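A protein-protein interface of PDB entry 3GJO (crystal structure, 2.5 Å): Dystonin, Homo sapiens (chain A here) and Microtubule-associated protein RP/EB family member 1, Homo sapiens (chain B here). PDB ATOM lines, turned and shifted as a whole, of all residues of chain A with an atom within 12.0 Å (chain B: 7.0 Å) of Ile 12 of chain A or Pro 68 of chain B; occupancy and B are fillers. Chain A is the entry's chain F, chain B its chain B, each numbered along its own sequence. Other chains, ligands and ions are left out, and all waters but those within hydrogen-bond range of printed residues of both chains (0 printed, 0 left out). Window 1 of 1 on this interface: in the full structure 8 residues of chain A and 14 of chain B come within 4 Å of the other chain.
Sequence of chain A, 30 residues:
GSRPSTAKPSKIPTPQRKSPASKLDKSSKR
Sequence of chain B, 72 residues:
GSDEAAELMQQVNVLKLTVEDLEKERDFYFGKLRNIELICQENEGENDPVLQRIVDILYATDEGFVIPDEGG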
ATOM      1  N   LYS A   8       4.804  26.387  -4.780  1.00  0.00           N
ATOM      2  CA  LYS A   8       4.938  27.314  -5.942  1.00  0.00           C
ATOM      3  C   LYS A   8       6.403  27.498  -6.395  1.00  0.00           C
ATOM      4  O   LYS A   8       6.787  26.949  -7.430  1.00  0.00           O
ATOM      5  CB  LYS A   8       4.257  28.658  -5.648  1.00  0.00           C
ATOM      6  CG  LYS A   8       2.755  28.572  -5.436  1.00  0.00           C
ATOM      7  CD  LYS A   8       2.250  29.750  -4.613  1.00  0.00           C
ATOM      8  CE  LYS A   8       0.746  29.959  -4.774  1.00  0.00           C
ATOM      9  NZ  LYS A   8      -0.072  28.761  -4.427  1.00  0.00           N
ATOM     10  N   PRO A   9       7.227  28.256  -5.628  1.00  0.00           N
ATOM     11  CA  PRO A   9       8.600  28.519  -6.063  1.00  0.00           C
ATOM     12  C   PRO A   9       9.623  27.580  -5.408  1.00  0.00           C
ATOM     13  O   PRO A   9       9.229  26.613  -4.755  1.00  0.00           O
ATOM     14  CB  PRO A   9       8.826  29.959  -5.585  1.00  0.00           C
ATOM     15  CG  PRO A   9       7.857  30.150  -4.408  1.00  0.00           C
ATOM     16  CD  PRO A   9       6.959  28.930  -4.343  1.00  0.00           C
ATOM     17  N   SER A  10      10.917  27.853  -5.597  1.00  0.00           N
ATOM     18  CA  SER A  10      11.977  27.127  -4.870  1.00  0.00           C
ATOM     19  C   SER A  10      12.363  27.847  -3.588  1.00  0.00           C
ATOM     20  O   SER A  10      12.288  29.074  -3.507  1.00  0.00           O
ATOM     21  CB  SER A  10      13.231  26.923  -5.725  1.00  0.00           C
ATOM     22  OG  SER A  10      14.237  26.213  -5.001  1.00  0.00           O
ATOM     23  N   LYS A  11      12.773  27.080  -2.587  1.00  0.00           N
ATOM     24  CA  LYS A  11      13.198  27.649  -1.317  1.00  0.00           C
ATOM     25  C   LYS A  11      14.474  26.954  -0.839  1.00  0.00           C
ATOM     26  O   LYS A  11      14.796  26.956   0.357  1.00  0.00           O
ATOM     27  CB  LYS A  11      12.066  27.557  -0.285  1.00  0.00           C
ATOM     28  CG  LYS A  11      10.943  28.556  -0.528  1.00  0.00           C
ATOM     29  CD  LYS A  11       9.593  28.083   0.007  1.00  0.00           C
ATOM     30  CE  LYS A  11       8.460  28.856  -0.681  1.00  0.00           C
ATOM     31  NZ  LYS A  11       7.087  28.546  -0.178  1.00  0.00           N
ATOM     32  N   ILE A  12      15.195  26.357  -1.791  1.00  0.00           N
ATOM     33  CA  ILE A  12      16.460  25.695  -1.507  1.00  0.00           C
ATOM     34  C   ILE A  12      17.546  26.760  -1.476  1.00  0.00           C
ATOM     35  O   ILE A  12      17.770  27.440  -2.478  1.00  0.00           O
ATOM     36  CB  ILE A  12      16.813  24.598  -2.548  1.00  0.00           C
ATOM     37  CG1 ILE A  12      15.793  23.452  -2.501  1.00  0.00           C
ATOM     38  CG2 ILE A  12      18.189  24.035  -2.271  1.00  0.00           C
ATOM     39  CD1 ILE A  12      15.890  22.468  -3.654  1.00  0.00           C
ATOM     40  N   PRO A  13      18.224  26.908  -0.322  1.00  0.00           N
ATOM     41  CA  PRO A  13      19.272  27.914  -0.147  1.00  0.00           C
ATOM     42  C   PRO A  13      20.294  27.898  -1.275  1.00  0.00           C
ATOM     43  O   PRO A  13      20.595  26.841  -1.832  1.00  0.00           O
ATOM     44  CB  PRO A  13      19.914  27.514   1.175  1.00  0.00           C
ATOM     45  CG  PRO A  13      18.817  26.871   1.920  1.00  0.00           C
ATOM     46  CD  PRO A  13      18.031  26.113   0.904  1.00  0.00           C
ATOM     47  N   THR A  14      20.801  29.077  -1.616  1.00  0.00           N
ATOM     48  CA  THR A  14      21.710  29.244  -2.740  1.00  0.00           C
ATOM     49  C   THR A  14      22.727  30.308  -2.315  1.00  0.00           C
ATOM     50  O   THR A  14      22.411  31.126  -1.450  1.00  0.00           O
ATOM     51  CB  THR A  14      20.928  29.685  -4.013  1.00  0.00           C
ATOM     52  OG1 THR A  14      19.656  29.027  -4.051  1.00  0.00           O
ATOM     53  CG2 THR A  14      21.689  29.328  -5.283  1.00  0.00           C
ATOM     54  N   PRO A  15      23.956  30.285  -2.886  1.00  0.00           N
ATOM     55  CA  PRO A  15      25.006  31.237  -2.484  1.00  0.00           C
ATOM     56  C   PRO A  15      24.691  32.724  -2.718  1.00  0.00           C
ATOM     57  O   PRO A  15      23.569  33.073  -3.089  1.00  0.00           O
ATOM     58  CB  PRO A  15      26.212  30.802  -3.332  1.00  0.00           C
ATOM     59  CG  PRO A  15      25.630  30.096  -4.487  1.00  0.00           C
ATOM     60  CD  PRO A  15      24.459  29.357  -3.916  1.00  0.00           C
ATOM     61  N   GLN A  16      25.706  33.569  -2.508  1.00  0.00           N
ATOM     62  CA  GLN A  16      25.609  35.043  -2.539  1.00  0.00           C
ATOM     63  C   GLN A  16      24.688  35.586  -1.450  1.00  0.00           C
ATOM     64  O   GLN A  16      24.761  35.149  -0.298  1.00  0.00           O
ATOM     65  CB  GLN A  16      25.213  35.582  -3.926  1.00  0.00           C
ATOM     66  CG  GLN A  16      26.298  35.419  -4.997  1.00  0.00           C
ATOM     67  CD  GLN A  16      26.181  36.428  -6.135  1.00  0.00           C
ATOM     68  OE1 GLN A  16      25.200  37.168  -6.234  1.00  0.00           O
ATOM     69  NE2 GLN A  16      27.193  36.460  -7.001  1.00  0.00           N
ATOM     70  N   PHE B  30      22.167  20.284  -7.491  1.00  0.00           N
ATOM     71  CA  PHE B  30      21.041  21.175  -7.267  1.00  0.00           C
ATOM     72  C   PHE B  30      19.778  20.693  -7.982  1.00  0.00           C
ATOM     73  O   PHE B  30      18.667  20.841  -7.458  1.00  0.00           O
ATOM     74  CB  PHE B  30      21.348  22.615  -7.662  1.00  0.00           C
ATOM     75  CG  PHE B  30      20.254  23.585  -7.297  1.00  0.00           C
ATOM     76  CD1 PHE B  30      20.178  24.115  -6.011  1.00  0.00           C
ATOM     77  CD2 PHE B  30      19.294  23.967  -8.237  1.00  0.00           C
ATOM     78  CE1 PHE B  30      19.171  25.023  -5.664  1.00  0.00           C
ATOM     79  CE2 PHE B  30      18.280  24.873  -7.905  1.00  0.00           C
ATOM     80  CZ  PHE B  30      18.213  25.399  -6.621  1.00  0.00           C
ATOM     81  N   GLY B  31      19.948  20.115  -9.167  1.00  0.00           N
ATOM     82  CA  GLY B  31      18.821  19.644  -9.950  1.00  0.00           C
ATOM     83  C   GLY B  31      18.085  18.539  -9.226  1.00  0.00           C
ATOM     84  O   GLY B  31      16.848  18.534  -9.173  1.00  0.00           O
ATOM     85  N   LYS B  32      18.844  17.603  -8.664  1.00  0.00           N
ATOM     86  CA  LYS B  32      18.268  16.501  -7.902  1.00  0.00           C
ATOM     87  C   LYS B  32      17.455  17.043  -6.739  1.00  0.00           C
ATOM     88  O   LYS B  32      16.368  16.541  -6.447  1.00  0.00           O
ATOM     89  CB  LYS B  32      19.370  15.559  -7.394  1.00  0.00           C
ATOM     90  CG  LYS B  32      20.039  14.782  -8.505  1.00  0.00           C
ATOM     91  CD  LYS B  32      21.295  14.080  -8.053  1.00  0.00           C
ATOM     92  CE  LYS B  32      21.751  13.065  -9.073  1.00  0.00           C
ATOM     93  NZ  LYS B  32      20.789  11.917  -9.249  1.00  0.00           N
ATOM     94  N   LEU B  33      17.987  18.073  -6.087  1.00  0.00           N
ATOM     95  CA  LEU B  33      17.328  18.690  -4.944  1.00  0.00           C
ATOM     96  C   LEU B  33      16.040  19.419  -5.320  1.00  0.00           C
ATOM     97  O   LEU B  33      15.087  19.416  -4.552  1.00  0.00           O
ATOM     98  CB  LEU B  33      18.271  19.654  -4.225  1.00  0.00           C
ATOM     99  CG  LEU B  33      19.515  19.064  -3.568  1.00  0.00           C
ATOM    100  CD1 LEU B  33      20.387  20.191  -3.097  1.00  0.00           C
ATOM    101  CD2 LEU B  33      19.143  18.160  -2.401  1.00  0.00           C
ATOM    102  N   ARG B  34      16.005  20.067  -6.479  1.00  0.00           N
ATOM    103  CA  ARG B  34      14.757  20.687  -6.914  1.00  0.00           C
ATOM    104  C   ARG B  34      13.679  19.648  -7.194  1.00  0.00           C
ATOM    105  O   ARG B  34      12.576  19.743  -6.665  1.00  0.00           O
ATOM    106  CB  ARG B  34      14.973  21.607  -8.105  1.00  0.00           C
ATOM    107  CG  ARG B  34      15.224  23.041  -7.680  1.00  0.00           C
ATOM    108  CD  ARG B  34      13.944  23.693  -7.154  1.00  0.00           C
ATOM    109  NE  ARG B  34      12.966  23.972  -8.213  1.00  0.00           N
ATOM    110  CZ  ARG B  34      11.679  24.257  -8.007  1.00  0.00           C
ATOM    111  NH1 ARG B  34      11.182  24.287  -6.774  1.00  0.00           N
ATOM    112  NH2 ARG B  34      10.879  24.498  -9.039  1.00  0.00           N
ATOM    113  N   ASN B  35      14.016  18.638  -7.992  1.00  0.00           N
ATOM    114  CA  ASN B  35      13.098  17.546  -8.273  1.00  0.00           C
ATOM    115  C   ASN B  35      12.532  16.921  -7.008  1.00  0.00           C
ATOM    116  O   ASN B  35      11.342  16.609  -6.949  1.00  0.00           O
ATOM    117  CB  ASN B  35      13.758  16.501  -9.165  1.00  0.00           C
ATOM    118  CG  ASN B  35      14.076  17.043 -10.552  1.00  0.00           C
ATOM    119  OD1 ASN B  35      13.400  17.943 -11.049  1.00  0.00           O
ATOM    120  ND2 ASN B  35      15.107  16.499 -11.178  1.00  0.00           N
ATOM    121  N   ILE B  36      13.377  16.775  -5.993  1.00  0.00           N
ATOM    122  CA  ILE B  36      12.946  16.262  -4.691  1.00  0.00           C
ATOM    123  C   ILE B  36      12.034  17.260  -3.970  1.00  0.00           C
ATOM    124  O   ILE B  36      10.974  16.877  -3.434  1.00  0.00           O
ATOM    125  CB  ILE B  36      14.146  15.832  -3.815  1.00  0.00           C
ATOM    126  CG1 ILE B  36      14.890  14.669  -4.501  1.00  0.00           C
ATOM    127  CG2 ILE B  36      13.671  15.423  -2.408  1.00  0.00           C
ATOM    128  CD1 ILE B  36      16.264  14.305  -3.914  1.00  0.00           C
ATOM    129  N   GLU B  37      12.430  18.533  -3.989  1.00  0.00           N
ATOM    130  CA  GLU B  37      11.578  19.615  -3.503  1.00  0.00           C
ATOM    131  C   GLU B  37      10.224  19.617  -4.222  1.00  0.00           C
ATOM    132  O   GLU B  37       9.203  19.865  -3.603  1.00  0.00           O
ATOM    133  CB  GLU B  37      12.265  20.983  -3.659  1.00  0.00           C
ATOM    134  CG  GLU B  37      11.402  22.158  -3.161  1.00  0.00           C
ATOM    135  CD  GLU B  37      12.071  23.515  -3.265  1.00  0.00           C
ATOM    136  OE1 GLU B  37      12.833  23.742  -4.228  1.00  0.00           O
ATOM    137  OE2 GLU B  37      11.827  24.370  -2.384  1.00  0.00           O
ATOM    138  N   LEU B  38      10.234  19.347  -5.527  1.00  0.00           N
ATOM    139  CA  LEU B  38       9.021  19.281  -6.321  1.00  0.00           C
ATOM    140  C   LEU B  38       8.029  18.247  -5.797  1.00  0.00           C
ATOM    141  O   LEU B  38       6.871  18.569  -5.555  1.00  0.00           O
ATOM    142  CB  LEU B  38       9.358  19.016  -7.792  1.00  0.00           C
ATOM    143  CG  LEU B  38       9.117  20.172  -8.770  1.00  0.00           C
ATOM    144  CD1 LEU B  38       9.322  21.541  -8.117  1.00  0.00           C
ATOM    145  CD2 LEU B  38       9.965  20.028 -10.043  1.00  0.00           C
ATOM    146  N   LEU B  58      16.384  19.784   2.913  1.00  0.00           N
ATOM    147  CA  LEU B  58      16.510  20.763   1.818  1.00  0.00           C
ATOM    148  C   LEU B  58      16.699  22.206   2.293  1.00  0.00           C
ATOM    149  O   LEU B  58      17.511  22.932   1.736  1.00  0.00           O
ATOM    150  CB  LEU B  58      15.316  20.711   0.859  1.00  0.00           C
ATOM    151  CG  LEU B  58      14.915  19.395   0.187  1.00  0.00           C
ATOM    152  CD1 LEU B  58      13.632  19.580  -0.607  1.00  0.00           C
ATOM    153  CD2 LEU B  58      15.994  18.868  -0.697  1.00  0.00           C
ATOM    154  N   TYR B  59      15.962  22.606   3.325  1.00  0.00           N
ATOM    155  CA  TYR B  59      15.891  24.019   3.712  1.00  0.00           C
ATOM    156  C   TYR B  59      16.896  24.486   4.755  1.00  0.00           C
ATOM    157  O   TYR B  59      16.934  25.677   5.090  1.00  0.00           O
ATOM    158  CB  TYR B  59      14.453  24.412   4.107  1.00  0.00           C
ATOM    159  CG  TYR B  59      13.479  24.298   2.950  1.00  0.00           C
ATOM    160  CD1 TYR B  59      13.938  24.307   1.629  1.00  0.00           C
ATOM    161  CD2 TYR B  59      12.116  24.181   3.168  1.00  0.00           C
ATOM    162  CE1 TYR B  59      13.076  24.190   0.562  1.00  0.00           C
ATOM    163  CE2 TYR B  59      11.228  24.080   2.098  1.00  0.00           C
ATOM    164  CZ  TYR B  59      11.721  24.084   0.799  1.00  0.00           C
ATOM    165  OH  TYR B  59      10.869  23.983  -0.265  1.00  0.00           O
ATOM    166  N   ALA B  60      17.710  23.553   5.251  1.00  0.00           N
ATOM    167  CA  ALA B  60      18.775  23.864   6.201  1.00  0.00           C
ATOM    168  C   ALA B  60      19.782  24.823   5.563  1.00  0.00           C
ATOM    169  O   ALA B  60      20.168  24.644   4.413  1.00  0.00           O
ATOM    170  CB  ALA B  60      19.451  22.596   6.650  1.00  0.00           C
ATOM    171  N   VAL B  66      21.550  31.630   1.330  1.00  0.00           N
ATOM    172  CA  VAL B  66      20.269  32.270   1.618  1.00  0.00           C
ATOM    173  C   VAL B  66      19.109  31.537   0.943  1.00  0.00           C
ATOM    174  O   VAL B  66      19.193  31.182  -0.234  1.00  0.00           O
ATOM    175  CB  VAL B  66      20.267  33.768   1.185  1.00  0.00           C
ATOM    176  CG1 VAL B  66      21.021  34.629   2.204  1.00  0.00           C
ATOM    177  CG2 VAL B  66      20.851  33.944  -0.228  1.00  0.00           C
ATOM    178  N   ILE B  67      18.032  31.309   1.691  1.00  0.00           N
ATOM    179  CA  ILE B  67      16.794  30.758   1.115  1.00  0.00           C
ATOM    180  C   ILE B  67      16.117  31.801   0.201  1.00  0.00           C
ATOM    181  O   ILE B  67      15.785  32.896   0.664  1.00  0.00           O
ATOM    182  CB  ILE B  67      15.809  30.213   2.213  1.00  0.00           C
ATOM    183  CG1 ILE B  67      14.417  29.938   1.612  1.00  0.00           C
ATOM    184  CG2 ILE B  67      15.760  31.152   3.428  1.00  0.00           C
ATOM    185  CD1 ILE B  67      13.336  29.477   2.607  1.00  0.00           C
ATOM    186  N   PRO B  68      15.928  31.473  -1.099  1.00  0.00           N
ATOM    187  CA  PRO B  68      15.380  32.448  -2.051  1.00  0.00           C
ATOM    188  C   PRO B  68      13.850  32.516  -2.014  1.00  0.00           C
ATOM    189  O   PRO B  68      13.276  33.008  -1.040  1.00  0.00           O
ATOM    190  CB  PRO B  68      15.862  31.926  -3.416  1.00  0.00           C
ATOM    191  CG  PRO B  68      16.606  30.628  -3.135  1.00  0.00           C
ATOM    192  CD  PRO B  68      16.208  30.193  -1.763  1.00  0.00           C
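The backbone NH of Val 66 of chain B is in hydrogen-bond range of the backbone carbonyl oxygen of Thr 14 of chain A, at 3.0 Å.
OE2 of Glu 37 of chain B is in hydrogen-bond range of N of Lys 11 of chain A (2.9 Å).
The side-chain hydroxyl (OG) of Ser 10 of chain A sits at hydrogen-bond distance from the side-chain carboxylate (OE1) of Glu 37 of chain B (2.9 Å).
The guanidinium group (NH1) of Arg 34 of chain B lies within salt-bridge range of the side-chain carboxylate (OE1) of Glu 37 of chain B (3.1 Å).
O of Ile 12 of chain A sits at hydrogen-bond distance from OG1 of Thr 14 of chain A, 2.9 Å away.
The side-chain hydroxyl (OG) of Ser 10 of chain A sits at hydrogen-bond distance from the backbone NH (N) of Ile 12 of chain A (3.4 Å).
Among the printed residues, pairs that only touch across the chains: Pro 9 of chain A with Arg 34 of chain B, Ser 10 of chain A with Arg 34 of chain B, Lys 11 of chain A with Tyr 59 of chain B, Lys 11 of chain A with Ile 67 of chain B, Lys 11 of chain A with Pro 68 of chain B, Ile 12 of chain A with Phe 30 of chain B, Ile 12 of chain A with Leu 33 of chain B, Ile 12 of chain A with Arg 34 of chain B, Ile 12 of chain A with Glu 37 of chain B, Ile 12 of chain A with Tyr 59 of chain B, Ile 12 of chain A with Pro 68 of chain B, Pro 13 of chain A with Leu 58 of chain B, Pro 13 of chain A with Tyr 59 of chain B, Pro 13 of chain A with Ala 60 of chain B, Pro 13 of chain A with Val 66 of chain B, Pro 13 of chain A with Ile 67 of chain B and Thr 14 of chain A with Pro 68 of chain B.
Ile 12 of chain A touches just these residues of chain B: Phe 30, Leu 33, Arg 34, Glu 37, Tyr 59 and Pro 68.
Of chain A, only Lys 11, Ile 12 and Thr 14 come within 4 Å of Pro 68 of chain B.
No residue of chain A comes within 4 Å of Gly 31 of chain B.
Leu 33 of chain B touches just one residue of chain A: Ile 12.
Arg 34 of chain B touches three residues of chain A.
Glu 37 of chain B touches three residues of chain A.
Of chain A, only Pro 13 comes within 4 Å of Leu 58 of chain B.
Printed residues of chain A within 4 Å of Val 66 of chain B: Pro 13 (3.3 Å) and Thr 14 (3.0 Å).
Of chain A, only Lys 11 and Pro 13 come within 4 Å of Ile 67 of chain B.
Printed residues of chain B within 4 Å of Ser 10 of chain A: Arg 34 and Glu 37.
Of the printed residues of chain B, Lys 11 of chain A touches Glu 37 (2.9 Å), Tyr 59 (3.1 Å), Ile 67 (3.3 Å) and Pro 68 (3.8 Å).
Of the printed residues of chain B, Pro 13 of chain A touches Leu 58 (3.3 Å), Tyr 59 (3.9 Å), Ala 60 (3.6 Å), Val 66 (3.3 Å) and Ile 67 (3.98 Å).
Of the printed residues of chain B, Thr 14 of chain A touches Val 66 (3.0 Å) and Pro 68 (3.6 Å).
The nearest residue of chain A that does not touch Pro 68 of chain B is Ser 10 of chain A (4.1 Å).
Of the 15 printed residues of chain B, 10 touch a printed residue of chain A.
Printed residues of chain B that touch a printed residue of chain A: Phe 30, Leu 33, Arg 34, Glu 37, Leu 58, Tyr 59, Ala 60, Val 66, Ile 67 and Pro 68.
Printed residues of chain A that touch a printed residue of chain B: Pro 9, Ser 10, Lys 11, Ile 12, Pro 13 and Thr 14.
Hydrophobic or aromatic side chains of chain A within 4 Å of the printed part of chain B: Ile 12 and Pro 13.
Among the printed residues, 20 pairs touch across the chains.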
